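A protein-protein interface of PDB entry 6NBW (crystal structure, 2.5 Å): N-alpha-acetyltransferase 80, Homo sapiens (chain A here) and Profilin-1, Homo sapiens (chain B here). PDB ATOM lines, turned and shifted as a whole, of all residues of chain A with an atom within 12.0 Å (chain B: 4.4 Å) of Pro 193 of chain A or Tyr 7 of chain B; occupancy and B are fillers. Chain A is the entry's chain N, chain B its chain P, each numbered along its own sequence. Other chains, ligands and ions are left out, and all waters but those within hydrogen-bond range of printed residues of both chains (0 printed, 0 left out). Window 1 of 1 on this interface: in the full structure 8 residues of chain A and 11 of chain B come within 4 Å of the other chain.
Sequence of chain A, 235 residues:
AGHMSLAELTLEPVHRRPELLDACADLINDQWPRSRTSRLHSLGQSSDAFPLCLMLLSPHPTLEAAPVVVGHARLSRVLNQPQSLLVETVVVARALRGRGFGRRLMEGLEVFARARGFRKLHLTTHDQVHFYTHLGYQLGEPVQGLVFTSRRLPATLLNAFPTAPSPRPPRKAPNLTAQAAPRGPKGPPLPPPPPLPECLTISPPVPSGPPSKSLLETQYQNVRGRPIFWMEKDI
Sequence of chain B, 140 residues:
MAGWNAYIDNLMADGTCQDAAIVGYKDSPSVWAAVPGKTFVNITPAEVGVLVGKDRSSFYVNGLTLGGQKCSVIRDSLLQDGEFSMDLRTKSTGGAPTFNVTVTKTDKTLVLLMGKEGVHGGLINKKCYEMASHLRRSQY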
ATOM      1  N   LEU A 190      20.636 -27.507 -18.583  1.00  0.00           N
ATOM      2  CA  LEU A 190      21.405 -27.422 -17.346  1.00  0.00           C
ATOM      3  C   LEU A 190      21.645 -25.963 -16.960  1.00  0.00           C
ATOM      4  O   LEU A 190      22.483 -25.295 -17.567  1.00  0.00           O
ATOM      5  CB  LEU A 190      22.742 -28.149 -17.495  1.00  0.00           C
ATOM      6  CG  LEU A 190      22.972 -29.310 -16.527  1.00  0.00           C
ATOM      7  CD1 LEU A 190      22.162 -30.524 -16.950  1.00  0.00           C
ATOM      8  CD2 LEU A 190      24.447 -29.646 -16.436  1.00  0.00           C
ATOM      9  N   PRO A 191      20.915 -25.463 -15.963  1.00  0.00           N
ATOM     10  CA  PRO A 191      21.116 -24.078 -15.547  1.00  0.00           C
ATOM     11  C   PRO A 191      22.544 -23.855 -15.106  1.00  0.00           C
ATOM     12  O   PRO A 191      23.192 -24.762 -14.547  1.00  0.00           O
ATOM     13  CB  PRO A 191      20.131 -23.913 -14.379  1.00  0.00           C
ATOM     14  CG  PRO A 191      19.110 -24.966 -14.575  1.00  0.00           C
ATOM     15  CD  PRO A 191      19.840 -26.118 -15.196  1.00  0.00           C
ATOM     16  N   PRO A 192      23.085 -22.657 -15.325  1.00  0.00           N
ATOM     17  CA  PRO A 192      24.432 -22.355 -14.838  1.00  0.00           C
ATOM     18  C   PRO A 192      24.459 -22.364 -13.323  1.00  0.00           C
ATOM     19  O   PRO A 192      23.501 -21.909 -12.679  1.00  0.00           O
ATOM     20  CB  PRO A 192      24.701 -20.949 -15.393  1.00  0.00           C
ATOM     21  CG  PRO A 192      23.342 -20.336 -15.482  1.00  0.00           C
ATOM     22  CD  PRO A 192      22.438 -21.468 -15.909  1.00  0.00           C
ATOM     23  N   PRO A 193      25.523 -22.870 -12.709  1.00  0.00           N
ATOM     24  CA  PRO A 193      25.586 -22.880 -11.251  1.00  0.00           C
ATOM     25  C   PRO A 193      25.800 -21.478 -10.717  1.00  0.00           C
ATOM     26  O   PRO A 193      26.583 -20.705 -11.290  1.00  0.00           O
ATOM     27  CB  PRO A 193      26.795 -23.779 -10.957  1.00  0.00           C
ATOM     28  CG  PRO A 193      27.679 -23.581 -12.126  1.00  0.00           C
ATOM     29  CD  PRO A 193      26.757 -23.410 -13.310  1.00  0.00           C
ATOM     30  N   PRO A 194      25.124 -21.102  -9.635  1.00  0.00           N
ATOM     31  CA  PRO A 194      25.452 -19.841  -8.979  1.00  0.00           C
ATOM     32  C   PRO A 194      26.816 -19.939  -8.322  1.00  0.00           C
ATOM     33  O   PRO A 194      27.397 -21.033  -8.246  1.00  0.00           O
ATOM     34  CB  PRO A 194      24.330 -19.675  -7.945  1.00  0.00           C
ATOM     35  CG  PRO A 194      23.935 -21.065  -7.619  1.00  0.00           C
ATOM     36  CD  PRO A 194      24.069 -21.834  -8.911  1.00  0.00           C
ATOM     37  N   PRO A 195      27.371 -18.829  -7.848  1.00  0.00           N
ATOM     38  CA  PRO A 195      28.730 -18.874  -7.300  1.00  0.00           C
ATOM     39  C   PRO A 195      28.774 -19.532  -5.929  1.00  0.00           C
ATOM     40  O   PRO A 195      27.816 -19.484  -5.153  1.00  0.00           O
ATOM     41  CB  PRO A 195      29.135 -17.395  -7.220  1.00  0.00           C
ATOM     42  CG  PRO A 195      28.107 -16.648  -8.033  1.00  0.00           C
ATOM     43  CD  PRO A 195      26.856 -17.452  -7.923  1.00  0.00           C
ATOM     44  N   LEU A 196      29.915 -20.162  -5.645  1.00  0.00           N
ATOM     45  CA  LEU A 196      30.160 -20.788  -4.356  1.00  0.00           C
ATOM     46  C   LEU A 196      30.442 -19.715  -3.309  1.00  0.00           C
ATOM     47  O   LEU A 196      30.656 -18.548  -3.643  1.00  0.00           O
ATOM     48  CB  LEU A 196      31.336 -21.756  -4.461  1.00  0.00           C
ATOM     49  CG  LEU A 196      31.031 -23.139  -5.036  1.00  0.00           C
ATOM     50  CD1 LEU A 196      32.325 -23.881  -5.325  1.00  0.00           C
ATOM     51  CD2 LEU A 196      30.148 -23.943  -4.089  1.00  0.00           C
ATOM     52  N   PRO A 197      30.445 -20.078  -2.025  1.00  0.00           N
ATOM     53  CA  PRO A 197      30.800 -19.093  -0.996  1.00  0.00           C
ATOM     54  C   PRO A 197      32.203 -18.542  -1.207  1.00  0.00           C
ATOM     55  O   PRO A 197      33.130 -19.270  -1.569  1.00  0.00           O
ATOM     56  CB  PRO A 197      30.698 -19.888   0.313  1.00  0.00           C
ATOM     57  CG  PRO A 197      30.757 -21.329  -0.098  1.00  0.00           C
ATOM     58  CD  PRO A 197      30.080 -21.377  -1.433  1.00  0.00           C
ATOM     59  N   GLU A 198      32.346 -17.240  -0.974  1.00  0.00           N
ATOM     60  CA  GLU A 198      33.635 -16.556  -1.066  1.00  0.00           C
ATOM     61  C   GLU A 198      34.406 -16.965  -2.319  1.00  0.00           C
ATOM     62  O   GLU A 198      35.546 -16.548  -2.526  1.00  0.00           O
ATOM     63  CB  GLU A 198      34.473 -16.840   0.186  1.00  0.00           C
ATOM     64  CG  GLU A 198      33.659 -17.131   1.451  1.00  0.00           C
ATOM     65  CD  GLU A 198      32.677 -16.028   1.817  1.00  0.00           C
ATOM     66  OE1 GLU A 198      32.162 -16.054   2.956  1.00  0.00           O
ATOM     67  OE2 GLU A 198      32.416 -15.141   0.976  1.00  0.00           O
ATOM     68  N   GLY B   3      32.007 -24.967 -13.514  1.00  0.00           N
ATOM     69  CA  GLY B   3      30.677 -25.515 -13.702  1.00  0.00           C
ATOM     70  C   GLY B   3      30.134 -26.166 -12.444  1.00  0.00           C
ATOM     71  O   GLY B   3      30.550 -25.832 -11.334  1.00  0.00           O
ATOM     72  N   TRP B   4      29.191 -27.097 -12.620  1.00  0.00           N
ATOM     73  CA  TRP B   4      28.669 -27.837 -11.476  1.00  0.00           C
ATOM     74  C   TRP B   4      29.724 -28.754 -10.876  1.00  0.00           C
ATOM     75  O   TRP B   4      29.672 -29.060  -9.681  1.00  0.00           O
ATOM     76  CB  TRP B   4      27.444 -28.653 -11.885  1.00  0.00           C
ATOM     77  CG  TRP B   4      26.240 -27.814 -12.112  1.00  0.00           C
ATOM     78  CD1 TRP B   4      25.655 -27.525 -13.308  1.00  0.00           C
ATOM     79  CD2 TRP B   4      25.473 -27.137 -11.113  1.00  0.00           C
ATOM     80  NE1 TRP B   4      24.564 -26.712 -13.115  1.00  0.00           N
ATOM     81  CE2 TRP B   4      24.431 -26.459 -11.775  1.00  0.00           C
ATOM     82  CE3 TRP B   4      25.566 -27.039  -9.721  1.00  0.00           C
ATOM     83  CZ2 TRP B   4      23.485 -25.694 -11.092  1.00  0.00           C
ATOM     84  CZ3 TRP B   4      24.628 -26.279  -9.046  1.00  0.00           C
ATOM     85  CH2 TRP B   4      23.602 -25.617  -9.731  1.00  0.00           C
ATOM     86  N   ASN B   5      30.679 -29.206 -11.691  1.00  0.00           N
ATOM     87  CA  ASN B   5      31.762 -30.027 -11.166  1.00  0.00           C
ATOM     88  C   ASN B   5      32.551 -29.284 -10.096  1.00  0.00           C
ATOM     89  O   ASN B   5      33.108 -29.910  -9.188  1.00  0.00           O
ATOM     90  CB  ASN B   5      32.672 -30.469 -12.308  1.00  0.00           C
ATOM     91  CG  ASN B   5      31.974 -31.405 -13.274  1.00  0.00           C
ATOM     92  OD1 ASN B   5      32.078 -32.626 -13.154  1.00  0.00           O
ATOM     93  ND2 ASN B   5      31.247 -30.838 -14.231  1.00  0.00           N
ATOM     94  N   ALA B   6      32.598 -27.952 -10.178  1.00  0.00           N
ATOM     95  CA  ALA B   6      33.203 -27.170  -9.106  1.00  0.00           C
ATOM     96  C   ALA B   6      32.513 -27.426  -7.772  1.00  0.00           C
ATOM     97  O   ALA B   6      33.147 -27.331  -6.714  1.00  0.00           O
ATOM     98  CB  ALA B   6      33.153 -25.682  -9.451  1.00  0.00           C
ATOM     99  N   TYR B   7      31.219 -27.753  -7.798  1.00  0.00           N
ATOM    100  CA  TYR B   7      30.511 -28.053  -6.558  1.00  0.00           C
ATOM    101  C   TYR B   7      30.891 -29.427  -6.026  1.00  0.00           C
ATOM    102  O   TYR B   7      30.987 -29.622  -4.809  1.00  0.00           O
ATOM    103  CB  TYR B   7      29.005 -27.953  -6.779  1.00  0.00           C
ATOM    104  CG  TYR B   7      28.490 -26.547  -6.623  1.00  0.00           C
ATOM    105  CD1 TYR B   7      28.900 -25.540  -7.485  1.00  0.00           C
ATOM    106  CD2 TYR B   7      27.603 -26.221  -5.608  1.00  0.00           C
ATOM    107  CE1 TYR B   7      28.439 -24.251  -7.342  1.00  0.00           C
ATOM    108  CE2 TYR B   7      27.136 -24.936  -5.458  1.00  0.00           C
ATOM    109  CZ  TYR B   7      27.556 -23.955  -6.328  1.00  0.00           C
ATOM    110  OH  TYR B   7      27.090 -22.670  -6.179  1.00  0.00           O
ATOM    111  N   ILE B   8      31.114 -30.392  -6.918  1.00  0.00           N
ATOM    112  CA  ILE B   8      31.630 -31.686  -6.484  1.00  0.00           C
ATOM    113  C   ILE B   8      33.017 -31.515  -5.881  1.00  0.00           C
ATOM    114  O   ILE B   8      33.327 -32.066  -4.819  1.00  0.00           O
ATOM    115  CB  ILE B   8      31.649 -32.682  -7.657  1.00  0.00           C
ATOM    116  CG1 ILE B   8      30.283 -32.725  -8.348  1.00  0.00           C
ATOM    117  CG2 ILE B   8      32.059 -34.062  -7.163  1.00  0.00           C
ATOM    118  CD1 ILE B   8      29.125 -32.997  -7.412  1.00  0.00           C
ATOM    119  N   ASP B   9      33.874 -30.750  -6.559  1.00  0.00           N
ATOM    120  CA  ASP B   9      35.180 -30.421  -6.000  1.00  0.00           C
ATOM    121  C   ASP B   9      35.034 -29.795  -4.619  1.00  0.00           C
ATOM    122  O   ASP B   9      35.737 -30.169  -3.674  1.00  0.00           O
ATOM    123  CB  ASP B   9      35.927 -29.472  -6.941  1.00  0.00           C
ATOM    124  CG  ASP B   9      36.360 -30.145  -8.233  1.00  0.00           C
ATOM    125  OD1 ASP B   9      36.639 -31.363  -8.211  1.00  0.00           O
ATOM    126  OD2 ASP B   9      36.426 -29.449  -9.271  1.00  0.00           O
ATOM    127  N   ASN B  10      34.114 -28.839  -4.485  1.00  0.00           N
ATOM    128  CA  ASN B  10      33.923 -28.160  -3.208  1.00  0.00           C
ATOM    129  C   ASN B  10      33.484 -29.142  -2.126  1.00  0.00           C
ATOM    130  O   ASN B  10      34.034 -29.154  -1.019  1.00  0.00           O
ATOM    131  CB  ASN B  10      32.895 -27.042  -3.377  1.00  0.00           C
ATOM    132  CG  ASN B  10      32.881 -26.078  -2.211  1.00  0.00           C
ATOM    133  OD1 ASN B  10      33.581 -25.066  -2.222  1.00  0.00           O
ATOM    134  ND2 ASN B  10      32.076 -26.382  -1.201  1.00  0.00           N
ATOM    135  N   LEU B  11      32.493 -29.980  -2.432  1.00  0.00           N
ATOM    136  CA  LEU B  11      31.977 -30.911  -1.434  1.00  0.00           C
ATOM    137  C   LEU B  11      32.997 -31.987  -1.081  1.00  0.00           C
ATOM    138  O   LEU B  11      32.969 -32.522   0.033  1.00  0.00           O
ATOM    139  CB  LEU B  11      30.684 -31.550  -1.942  1.00  0.00           C
ATOM    140  CG  LEU B  11      29.492 -30.609  -2.136  1.00  0.00           C
ATOM    141  CD1 LEU B  11      28.417 -31.255  -3.002  1.00  0.00           C
ATOM    142  CD2 LEU B  11      28.913 -30.196  -0.788  1.00  0.00           C
ATOM    143  N   ILE B  22      25.005 -33.610  -7.691  1.00  0.00           N
ATOM    144  CA  ILE B  22      23.894 -32.675  -7.789  1.00  0.00           C
ATOM    145  C   ILE B  22      22.993 -33.188  -8.900  1.00  0.00           C
ATOM    146  O   ILE B  22      23.449 -33.379 -10.034  1.00  0.00           O
ATOM    147  CB  ILE B  22      24.373 -31.242  -8.064  1.00  0.00           C
ATOM    148  CG1 ILE B  22      25.284 -30.790  -6.920  1.00  0.00           C
ATOM    149  CG2 ILE B  22      23.189 -30.294  -8.226  1.00  0.00           C
ATOM    150  CD1 ILE B  22      25.600 -29.317  -6.919  1.00  0.00           C
ATOM    151  N   MET B 131      25.243 -26.896   2.066  1.00  0.00           N
ATOM    152  CA  MET B 131      25.288 -26.694   0.621  1.00  0.00           C
ATOM    153  C   MET B 131      23.894 -26.438   0.060  1.00  0.00           C
ATOM    154  O   MET B 131      23.718 -25.589  -0.823  1.00  0.00           O
ATOM    155  CB  MET B 131      25.923 -27.907  -0.057  1.00  0.00           C
ATOM    156  CG  MET B 131      25.897 -27.855  -1.579  1.00  0.00           C
ATOM    157  SD  MET B 131      26.723 -26.400  -2.260  1.00  0.00           S
ATOM    158  CE  MET B 131      28.435 -26.793  -1.921  1.00  0.00           C
ATOM    159  N   HIS B 134      22.843 -22.947   0.860  1.00  0.00           N
ATOM    160  CA  HIS B 134      23.528 -22.035  -0.050  1.00  0.00           C
ATOM    161  C   HIS B 134      22.850 -22.000  -1.415  1.00  0.00           C
ATOM    162  O   HIS B 134      22.783 -20.944  -2.056  1.00  0.00           O
ATOM    163  CB  HIS B 134      24.993 -22.451  -0.184  1.00  0.00           C
ATOM    164  CG  HIS B 134      25.721 -21.771  -1.303  1.00  0.00           C
ATOM    165  ND1 HIS B 134      25.995 -20.420  -1.302  1.00  0.00           N
ATOM    166  CD2 HIS B 134      26.242 -22.260  -2.453  1.00  0.00           C
ATOM    167  CE1 HIS B 134      26.650 -20.107  -2.406  1.00  0.00           C
ATOM    168  NE2 HIS B 134      26.812 -21.204  -3.122  1.00  0.00           N
ATOM    169  N   LEU B 135      22.336 -23.142  -1.877  1.00  0.00           N
ATOM    170  CA  LEU B 135      21.707 -23.184  -3.194  1.00  0.00           C
ATOM    171  C   LEU B 135      20.295 -22.607  -3.162  1.00  0.00           C
ATOM    172  O   LEU B 135      19.878 -21.937  -4.113  1.00  0.00           O
ATOM    173  CB  LEU B 135      21.695 -24.617  -3.730  1.00  0.00           C
ATOM    174  CG  LEU B 135      23.049 -25.116  -4.251  1.00  0.00           C
ATOM    175  CD1 LEU B 135      22.977 -26.574  -4.677  1.00  0.00           C
ATOM    176  CD2 LEU B 135      23.540 -24.250  -5.405  1.00  0.00           C
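A ring nitrogen (NE2) of His 134 of chain B is in hydrogen-bond range of the side-chain hydroxyl (OH) of Tyr 7 of chain B (3.4 Å).
Printed residues of chain B within 4 Å of Leu 190 of chain A: Trp 4 (3.97 Å).
Of the printed residues of chain B, Pro 191 of chain A touches Trp 4.
Pro 192 of chain A touches none of the printed residues of chain B.
Of the printed residues of chain B, Pro 193 of chain A touches Gly 3, Trp 4 and Tyr 7.
Of the printed residues of chain B, Pro 194 of chain A touches Trp 4, Tyr 7 and Leu 135.
Of the printed residues of chain B, Leu 196 of chain A touches Ala 6 (3.8 Å), Tyr 7 (3.4 Å), Asn 10 (3.6 Å), Met 131 (3.97 Å) and His 134 (3.6 Å).
Of the printed residues of chain B, Pro 197 of chain A touches His 134.
Glu 198 of chain A touches none of the printed residues of chain B.
No residue of chain A comes within 4 Å of Asn 5 of chain B.
Ala 6 of chain B touches one residue of chain A.
Of the printed residues of chain A, Tyr 7 of chain B touches Pro 193, Pro 194, Pro 195 and Leu 196.
No residue of chain A comes within 4 Å of Ile 8 of chain B.
No residue of chain A comes within 4 Å of Asp 9 of chain B.
Asn 10 of chain B touches one residue of chain A.
No residue of chain A comes within 4 Å of Leu 11 of chain B.
Leu 135 of chain B touches one residue of chain A.
The nearest printed residue of chain B that does not touch Pro 193 of chain A is Leu 135 of chain B (6.3 Å).
The nearest printed residue of chain A that does not touch Tyr 7 of chain B is Pro 197 of chain A (5.8 Å).
The nearest printed residue of chain B that does not touch Leu 190 of chain A is Asn 5 of chain B (7.2 Å).
Among the printed residues, merely in contact across the chains: Leu 190 of chain A with Trp 4 of chain B (3.97 Å), Pro 193 of chain A with Gly 3 of chain B (3.6 Å), Pro 193 of chain A with Trp 4 of chain B (3.5 Å), Pro 193 of chain A with Tyr 7 of chain B (3.999 Å), Pro 194 of chain A with Trp 4 of chain B (3.9 Å), Pro 194 of chain A with Leu 135 of chain B (3.9 Å), Leu 196 of chain A with Ala 6 of chain B (3.8 Å), Leu 196 of chain A with Tyr 7 of chain B (3.4 Å), Leu 196 of chain A with Asn 10 of chain B (3.6 Å), Leu 196 of chain A with Met 131 of chain B (3.97 Å), Leu 196 of chain A with His 134 of chain B (3.6 Å) and Pro 197 of chain A with His 134 of chain B (3.7 Å).
Of the 9 printed residues of chain A, 7 touch a printed residue of chain B.
Hydrophobic or aromatic side chains of chain A that line the printed part of chain B: Leu 190, Pro 193, Pro 194, Leu 196 and Pro 197.
Along chain A the printed residues that touch a printed residue of chain B span positions 190 to 197.
Hydrophobic or aromatic side chains of chain B within 4 Å of the printed part of chain A: Trp 4, Tyr 7, Met 131, His 134 and Leu 135.
The backbone carbonyl oxygen (O) of Pro 191 of chain A sits at hydrogen-bond distance from the indole nitrogen (NE1) of Trp 4 of chain B (2.8 Å).
The backbone carbonyl oxygen of Pro 194 of chain A lies within hydrogen-bond range of the side-chain hydroxyl of Tyr 7 of chain B (2.7 Å).
The side-chain hydroxyl (OH) of Tyr 7 of chain B lies within hydrogen-bond range of the backbone carbonyl oxygen (O) of Pro 195 of chain A, at 3.4 Å.
The backbone carbonyl oxygen (O) of Pro 195 of chain A sits at hydrogen-bond distance from a ring nitrogen (NE2) of His 134 of chain B.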
